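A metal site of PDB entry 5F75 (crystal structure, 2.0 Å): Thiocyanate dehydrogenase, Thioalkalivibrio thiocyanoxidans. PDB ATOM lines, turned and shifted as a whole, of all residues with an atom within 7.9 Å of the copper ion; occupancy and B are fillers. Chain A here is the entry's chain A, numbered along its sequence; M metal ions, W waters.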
ATOM      1  N   LYS A 103     -17.012  14.856  18.805  1.00  0.00           N
ATOM      2  CA  LYS A 103     -17.843  14.910  17.581  1.00  0.00           C
ATOM      3  C   LYS A 103     -19.105  15.749  17.844  1.00  0.00           C
ATOM      4  O   LYS A 103     -18.954  16.935  18.172  1.00  0.00           O
ATOM      5  CB  LYS A 103     -18.185  13.492  17.122  1.00  0.00           C
ATOM      6  CG  LYS A 103     -18.722  13.360  15.718  1.00  0.00           C
ATOM      7  CD  LYS A 103     -17.608  13.240  14.709  1.00  0.00           C
ATOM      8  CE  LYS A 103     -18.211  13.267  13.312  1.00  0.00           C
ATOM      9  NZ  LYS A 103     -17.261  12.893  12.242  1.00  0.00           N
ATOM     10  N   ILE A 133     -18.092  20.350  15.560  1.00  0.00           N
ATOM     11  CA  ILE A 133     -17.987  18.895  15.405  1.00  0.00           C
ATOM     12  C   ILE A 133     -16.514  18.571  15.637  1.00  0.00           C
ATOM     13  O   ILE A 133     -15.688  18.532  14.711  1.00  0.00           O
ATOM     14  CB  ILE A 133     -18.549  18.378  14.027  1.00  0.00           C
ATOM     15  CG1 ILE A 133     -20.058  18.677  13.891  1.00  0.00           C
ATOM     16  CG2 ILE A 133     -18.288  16.853  13.877  1.00  0.00           C
ATOM     17  CD1 ILE A 133     -20.602  18.487  12.454  1.00  0.00           C
ATOM     18  N   MET A 134     -16.169  18.376  16.904  1.00  0.00           N
ATOM     19  CA  MET A 134     -14.793  18.181  17.313  1.00  0.00           C
ATOM     20  C   MET A 134     -14.380  16.789  16.800  1.00  0.00           C
ATOM     21  O   MET A 134     -14.985  15.765  17.176  1.00  0.00           O
ATOM     22  CB  MET A 134     -14.685  18.285  18.850  1.00  0.00           C
ATOM     23  CG  MET A 134     -15.366  19.539  19.409  1.00  0.00           C
ATOM     24  SD  MET A 134     -14.419  20.989  18.889  1.00  0.00           S
ATOM     25  CE  MET A 134     -13.152  20.826  20.172  1.00  0.00           C
ATOM     26  N   HIS A 135     -13.343  16.748  15.949  1.00  0.00           N
ATOM     27  CA  HIS A 135     -13.119  15.591  15.108  1.00  0.00           C
ATOM     28  C   HIS A 135     -11.880  14.765  15.415  1.00  0.00           C
ATOM     29  O   HIS A 135     -11.915  13.855  16.273  1.00  0.00           O
ATOM     30  CB  HIS A 135     -13.204  15.981  13.618  1.00  0.00           C
ATOM     31  CG  HIS A 135     -13.542  14.815  12.744  1.00  0.00           C
ATOM     32  ND1 HIS A 135     -13.302  14.791  11.393  1.00  0.00           N
ATOM     33  CD2 HIS A 135     -14.063  13.607  13.060  1.00  0.00           C
ATOM     34  CE1 HIS A 135     -13.670  13.610  10.903  1.00  0.00           C
ATOM     35  NE2 HIS A 135     -14.132  12.878  11.889  1.00  0.00           N
ATOM     36  N   HIS A 136     -10.794  15.020  14.724  1.00  0.00           N
ATOM     37  CA  HIS A 136      -9.547  14.315  15.067  1.00  0.00           C
ATOM     38  C   HIS A 136      -8.579  15.106  15.944  1.00  0.00           C
ATOM     39  O   HIS A 136      -8.713  16.342  16.069  1.00  0.00           O
ATOM     40  CB  HIS A 136      -8.893  13.807  13.798  1.00  0.00           C
ATOM     41  CG  HIS A 136      -9.730  12.756  13.129  1.00  0.00           C
ATOM     42  ND1 HIS A 136      -9.833  11.466  13.615  1.00  0.00           N
ATOM     43  CD2 HIS A 136     -10.532  12.801  12.031  1.00  0.00           C
ATOM     44  CE1 HIS A 136     -10.661  10.776  12.846  1.00  0.00           C
ATOM     45  NE2 HIS A 136     -11.088  11.558  11.871  1.00  0.00           N
ATOM     46  N   GLN A 156     -15.278  19.589  11.819  1.00  0.00           N
ATOM     47  CA  GLN A 156     -15.994  19.603  10.553  1.00  0.00           C
ATOM     48  C   GLN A 156     -17.271  20.396  10.642  1.00  0.00           C
ATOM     49  O   GLN A 156     -17.812  20.616  11.733  1.00  0.00           O
ATOM     50  CB  GLN A 156     -16.377  18.162  10.102  1.00  0.00           C
ATOM     51  CG  GLN A 156     -15.183  17.291   9.774  1.00  0.00           C
ATOM     52  CD  GLN A 156     -15.580  15.829   9.501  1.00  0.00           C
ATOM     53  OE1 GLN A 156     -16.341  15.206  10.257  1.00  0.00           O
ATOM     54  NE2 GLN A 156     -15.009  15.257   8.444  1.00  0.00           N
ATOM     55  N   ASN A 160     -21.588  17.940   6.916  1.00  0.00           N
ATOM     56  CA  ASN A 160     -21.274  16.867   7.896  1.00  0.00           C
ATOM     57  C   ASN A 160     -22.228  16.879   9.116  1.00  0.00           C
ATOM     58  O   ASN A 160     -22.427  15.862   9.770  1.00  0.00           O
ATOM     59  CB  ASN A 160     -19.855  16.972   8.378  1.00  0.00           C
ATOM     60  CG  ASN A 160     -18.844  16.726   7.278  1.00  0.00           C
ATOM     61  OD1 ASN A 160     -18.642  15.588   6.849  1.00  0.00           O
ATOM     62  ND2 ASN A 160     -18.142  17.779   6.877  1.00  0.00           N
ATOM     63  N   TYR A 164     -25.712  11.933  10.354  1.00  0.00           N
ATOM     64  CA  TYR A 164     -25.862  10.920  11.455  1.00  0.00           C
ATOM     65  C   TYR A 164     -27.325  10.863  11.877  1.00  0.00           C
ATOM     66  O   TYR A 164     -28.127  11.651  11.380  1.00  0.00           O
ATOM     67  CB  TYR A 164     -24.920  11.227  12.663  1.00  0.00           C
ATOM     68  CG  TYR A 164     -23.451  11.210  12.244  1.00  0.00           C
ATOM     69  CD1 TYR A 164     -22.839  12.370  11.732  1.00  0.00           C
ATOM     70  CD2 TYR A 164     -22.698  10.030  12.277  1.00  0.00           C
ATOM     71  CE1 TYR A 164     -21.520  12.362  11.271  1.00  0.00           C
ATOM     72  CE2 TYR A 164     -21.363  10.011  11.829  1.00  0.00           C
ATOM     73  CZ  TYR A 164     -20.779  11.177  11.323  1.00  0.00           C
ATOM     74  OH  TYR A 164     -19.472  11.203  10.868  1.00  0.00           O
ATOM     75  N   GLY A 204     -10.166  19.047   7.771  1.00  0.00           N
ATOM     76  CA  GLY A 204     -11.152  18.457   8.674  1.00  0.00           C
ATOM     77  C   GLY A 204     -11.106  16.967   8.988  1.00  0.00           C
ATOM     78  O   GLY A 204     -12.037  16.463   9.668  1.00  0.00           O
ATOM     79  N   VAL A 205     -10.075  16.251   8.517  1.00  0.00           N
ATOM     80  CA  VAL A 205      -9.910  14.806   8.848  1.00  0.00           C
ATOM     81  C   VAL A 205      -8.677  14.548   9.710  1.00  0.00           C
ATOM     82  O   VAL A 205      -8.508  15.252  10.707  1.00  0.00           O
ATOM     83  CB  VAL A 205      -9.961  13.889   7.592  1.00  0.00           C
ATOM     84  CG1 VAL A 205     -10.240  12.425   7.986  1.00  0.00           C
ATOM     85  CG2 VAL A 205     -11.066  14.376   6.694  1.00  0.00           C
ATOM     86  N   HIS A 206      -7.812  13.590   9.378  1.00  0.00           N
ATOM     87  CA  HIS A 206      -6.884  13.094  10.417  1.00  0.00           C
ATOM     88  C   HIS A 206      -5.822  14.073  10.797  1.00  0.00           C
ATOM     89  O   HIS A 206      -5.281  14.763   9.928  1.00  0.00           O
ATOM     90  CB  HIS A 206      -6.267  11.720  10.111  1.00  0.00           C
ATOM     91  CG  HIS A 206      -7.260  10.584  10.169  1.00  0.00           C
ATOM     92  ND1 HIS A 206      -7.715  10.051  11.359  1.00  0.00           N
ATOM     93  CD2 HIS A 206      -7.951   9.960   9.194  1.00  0.00           C
ATOM     94  CE1 HIS A 206      -8.607   9.121  11.109  1.00  0.00           C
ATOM     95  NE2 HIS A 206      -8.761   9.024   9.807  1.00  0.00           N
ATOM     96  N   GLU A 288     -17.518  14.354   4.443  1.00  0.00           N
ATOM     97  CA  GLU A 288     -16.506  13.323   4.327  1.00  0.00           C
ATOM     98  C   GLU A 288     -17.244  12.003   4.134  1.00  0.00           C
ATOM     99  O   GLU A 288     -18.273  11.738   4.826  1.00  0.00           O
ATOM    100  CB  GLU A 288     -15.670  13.251   5.620  1.00  0.00           C
ATOM    101  CG  GLU A 288     -14.721  12.070   5.814  1.00  0.00           C
ATOM    102  CD  GLU A 288     -14.414  11.867   7.300  1.00  0.00           C
ATOM    103  OE1 GLU A 288     -14.914  12.648   8.139  1.00  0.00           O
ATOM    104  OE2 GLU A 288     -13.715  10.912   7.661  1.00  0.00           O
ATOM    105  N   LEU A 289     -16.701  11.163   3.256  1.00  0.00           N
ATOM    106  CA  LEU A 289     -17.301   9.860   2.970  1.00  0.00           C
ATOM    107  C   LEU A 289     -17.400   9.038   4.278  1.00  0.00           C
ATOM    108  O   LEU A 289     -16.402   8.886   4.996  1.00  0.00           O
ATOM    109  CB  LEU A 289     -16.401   9.120   1.989  1.00  0.00           C
ATOM    110  CG  LEU A 289     -16.339   9.767   0.608  1.00  0.00           C
ATOM    111  CD1 LEU A 289     -15.621   8.818  -0.339  1.00  0.00           C
ATOM    112  CD2 LEU A 289     -17.723  10.139   0.053  1.00  0.00           C
ATOM    113  N   PRO A 291     -17.889   5.358   6.411  1.00  0.00           N
ATOM    114  CA  PRO A 291     -17.280   4.048   6.105  1.00  0.00           C
ATOM    115  C   PRO A 291     -18.182   3.343   5.106  1.00  0.00           C
ATOM    116  O   PRO A 291     -19.419   3.410   5.236  1.00  0.00           O
ATOM    117  CB  PRO A 291     -17.291   3.316   7.470  1.00  0.00           C
ATOM    118  CG  PRO A 291     -17.381   4.415   8.490  1.00  0.00           C
ATOM    119  CD  PRO A 291     -18.229   5.479   7.841  1.00  0.00           C
ATOM    120  N   PHE A 436     -11.065   0.643  10.480  1.00  0.00           N
ATOM    121  CA  PHE A 436     -10.494   1.951  10.089  1.00  0.00           C
ATOM    122  C   PHE A 436      -9.607   2.637  11.132  1.00  0.00           C
ATOM    123  O   PHE A 436      -9.167   3.806  10.950  1.00  0.00           O
ATOM    124  CB  PHE A 436     -11.563   2.860   9.446  1.00  0.00           C
ATOM    125  CG  PHE A 436     -12.683   3.265  10.373  1.00  0.00           C
ATOM    126  CD1 PHE A 436     -12.538   4.363  11.252  1.00  0.00           C
ATOM    127  CD2 PHE A 436     -13.888   2.616  10.343  1.00  0.00           C
ATOM    128  CE1 PHE A 436     -13.557   4.765  12.106  1.00  0.00           C
ATOM    129  CE2 PHE A 436     -14.922   3.012  11.203  1.00  0.00           C
ATOM    130  CZ  PHE A 436     -14.756   4.075  12.082  1.00  0.00           C
ATOM    131  N   HIS A 437      -9.305   1.920  12.206  1.00  0.00           N
ATOM    132  CA  HIS A 437      -8.344   2.405  13.201  1.00  0.00           C
ATOM    133  C   HIS A 437      -7.480   1.289  13.720  1.00  0.00           C
ATOM    134  O   HIS A 437      -7.903   0.165  13.742  1.00  0.00           O
ATOM    135  CB  HIS A 437      -9.050   3.052  14.395  1.00  0.00           C
ATOM    136  CG  HIS A 437      -9.879   4.239  14.040  1.00  0.00           C
ATOM    137  ND1 HIS A 437      -9.331   5.453  13.679  1.00  0.00           N
ATOM    138  CD2 HIS A 437     -11.227   4.388  13.972  1.00  0.00           C
ATOM    139  CE1 HIS A 437     -10.320   6.312  13.445  1.00  0.00           C
ATOM    140  NE2 HIS A 437     -11.472   5.694  13.604  1.00  0.00           N
ATOM    141  N   HIS A 482     -14.915   3.301  17.506  1.00  0.00           N
ATOM    142  CA  HIS A 482     -13.908   4.152  16.866  1.00  0.00           C
ATOM    143  C   HIS A 482     -12.437   3.894  17.207  1.00  0.00           C
ATOM    144  O   HIS A 482     -11.951   2.797  17.012  1.00  0.00           O
ATOM    145  CB  HIS A 482     -14.355   5.610  16.931  1.00  0.00           C
ATOM    146  CG  HIS A 482     -15.536   5.850  16.080  1.00  0.00           C
ATOM    147  ND1 HIS A 482     -15.442   6.123  14.729  1.00  0.00           N
ATOM    148  CD2 HIS A 482     -16.857   5.757  16.357  1.00  0.00           C
ATOM    149  CE1 HIS A 482     -16.658   6.246  14.219  1.00  0.00           C
ATOM    150  NE2 HIS A 482     -17.534   6.023  15.188  1.00  0.00           N
ATOM    151  N   GLN A 501     -23.478   8.837  17.550  1.00  0.00           N
ATOM    152  CA  GLN A 501     -23.894  10.190  18.026  1.00  0.00           C
ATOM    153  C   GLN A 501     -25.250  10.283  18.654  1.00  0.00           C
ATOM    154  O   GLN A 501     -25.655  11.369  19.007  1.00  0.00           O
ATOM    155  CB  GLN A 501     -23.882  11.245  16.905  1.00  0.00           C
ATOM    156  CG  GLN A 501     -22.619  11.209  16.026  1.00  0.00           C
ATOM    157  CD  GLN A 501     -21.345  11.401  16.840  1.00  0.00           C
ATOM    158  OE1 GLN A 501     -21.207  12.371  17.601  1.00  0.00           O
ATOM    159  NE2 GLN A 501     -20.403  10.465  16.675  1.00  0.00           N
ATOM    160  N   GLY A 526     -19.156  11.563  21.372  1.00  0.00           N
ATOM    161  CA  GLY A 526     -19.238  10.816  20.105  1.00  0.00           C
ATOM    162  C   GLY A 526     -17.880  10.562  19.458  1.00  0.00           C
ATOM    163  O   GLY A 526     -17.791  10.406  18.231  1.00  0.00           O
ATOM    164  N   HIS A 527     -16.842  10.553  20.297  1.00  0.00           N
ATOM    165  CA  HIS A 527     -15.435  10.368  19.907  1.00  0.00           C
ATOM    166  C   HIS A 527     -15.205   9.667  18.589  1.00  0.00           C
ATOM    167  O   HIS A 527     -15.563   8.462  18.434  1.00  0.00           O
ATOM    168  CB  HIS A 527     -14.620   9.586  20.973  1.00  0.00           C
ATOM    169  CG  HIS A 527     -15.371   9.278  22.233  1.00  0.00           C
ATOM    170  ND1 HIS A 527     -16.353   8.316  22.289  1.00  0.00           N
ATOM    171  CD2 HIS A 527     -15.266   9.798  23.479  1.00  0.00           C
ATOM    172  CE1 HIS A 527     -16.814   8.243  23.532  1.00  0.00           C
ATOM    173  NE2 HIS A 527     -16.177   9.138  24.269  1.00  0.00           N
ATOM    174  N   HIS A 528     -14.576  10.389  17.653  1.00  0.00           N
ATOM    175  CA  HIS A 528     -13.921   9.747  16.487  1.00  0.00           C
ATOM    176  C   HIS A 528     -12.409   9.699  16.581  1.00  0.00           C
ATOM    177  O   HIS A 528     -11.712   9.431  15.595  1.00  0.00           O
ATOM    178  CB  HIS A 528     -14.351  10.363  15.169  1.00  0.00           C
ATOM    179  CG  HIS A 528     -15.739   9.990  14.766  1.00  0.00           C
ATOM    180  ND1 HIS A 528     -16.225  10.158  13.500  1.00  0.00           N
ATOM    181  CD2 HIS A 528     -16.741   9.434  15.483  1.00  0.00           C
ATOM    182  CE1 HIS A 528     -17.486   9.766  13.452  1.00  0.00           C
ATOM    183  NE2 HIS A 528     -17.817   9.292  14.635  1.00  0.00           N
ATOM    184  N   ASP A 529     -11.888   9.953  17.768  1.00  0.00           N
ATOM    185  CA  ASP A 529     -10.436   9.883  18.002  1.00  0.00           C
ATOM    186  C   ASP A 529     -10.204   9.813  19.510  1.00  0.00           C
ATOM    187  O   ASP A 529     -11.090  10.154  20.292  1.00  0.00           O
ATOM    188  CB  ASP A 529      -9.720  11.144  17.422  1.00  0.00           C
ATOM    189  CG  ASP A 529      -8.459  10.787  16.693  1.00  0.00           C
ATOM    190  OD1 ASP A 529      -7.807   9.862  17.196  1.00  0.00           O
ATOM    191  OD2 ASP A 529      -8.135  11.378  15.612  1.00  0.00           O
HETATM  192 CU    CU M   1     -15.585  11.471  12.129  1.00  0.00          CU
HETATM  193  O   HOH W   1     -14.222  10.328  11.842  1.00  0.00           O
HETATM  194  O   HOH W   2     -15.892  11.067  10.095  1.00  0.00           O
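O of His 528 lies close to ND1 of His 136 (3.4 Å).
The side-chain amide oxygen (OE1) of Gln 156 sits close to the side-chain amino group (NZ) of Lys 103 (3.2 Å).
ND1 of His 135 sits at hydrogen-bond distance from O of Gly 204 (2.7 Å).
A ring nitrogen (NE2) of His 528 sits at hydrogen-bond distance from the side-chain amide nitrogen (NE2) of Gln 501, 3.5 Å away.
A ring nitrogen (NE2) of His 135 lies close to a ring nitrogen (NE2) of His 136.
A ring nitrogen (NE2) of His 482 lies close to a ring nitrogen (NE2) of His 528 (3.3 Å).
N of Lys 103 is in hydrogen-bond range of O of Met 134 (2.8 Å).
OE1 of Gln 156 sits close to ND1 of His 135 (3.3 Å).
Three residues have an atom within 4 Å of the copper ion: Lys 103, His 135 and His 528.
The copper ion is bound by water W1 (1.8 Å), ND1 of His 528 (2.0 Å), NE2 of His 135 (2.0 Å), water W2 (2.1 Å) and NZ of Lys 103 (2.2 Å).
The copper ion has five donor atoms within binding distance.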
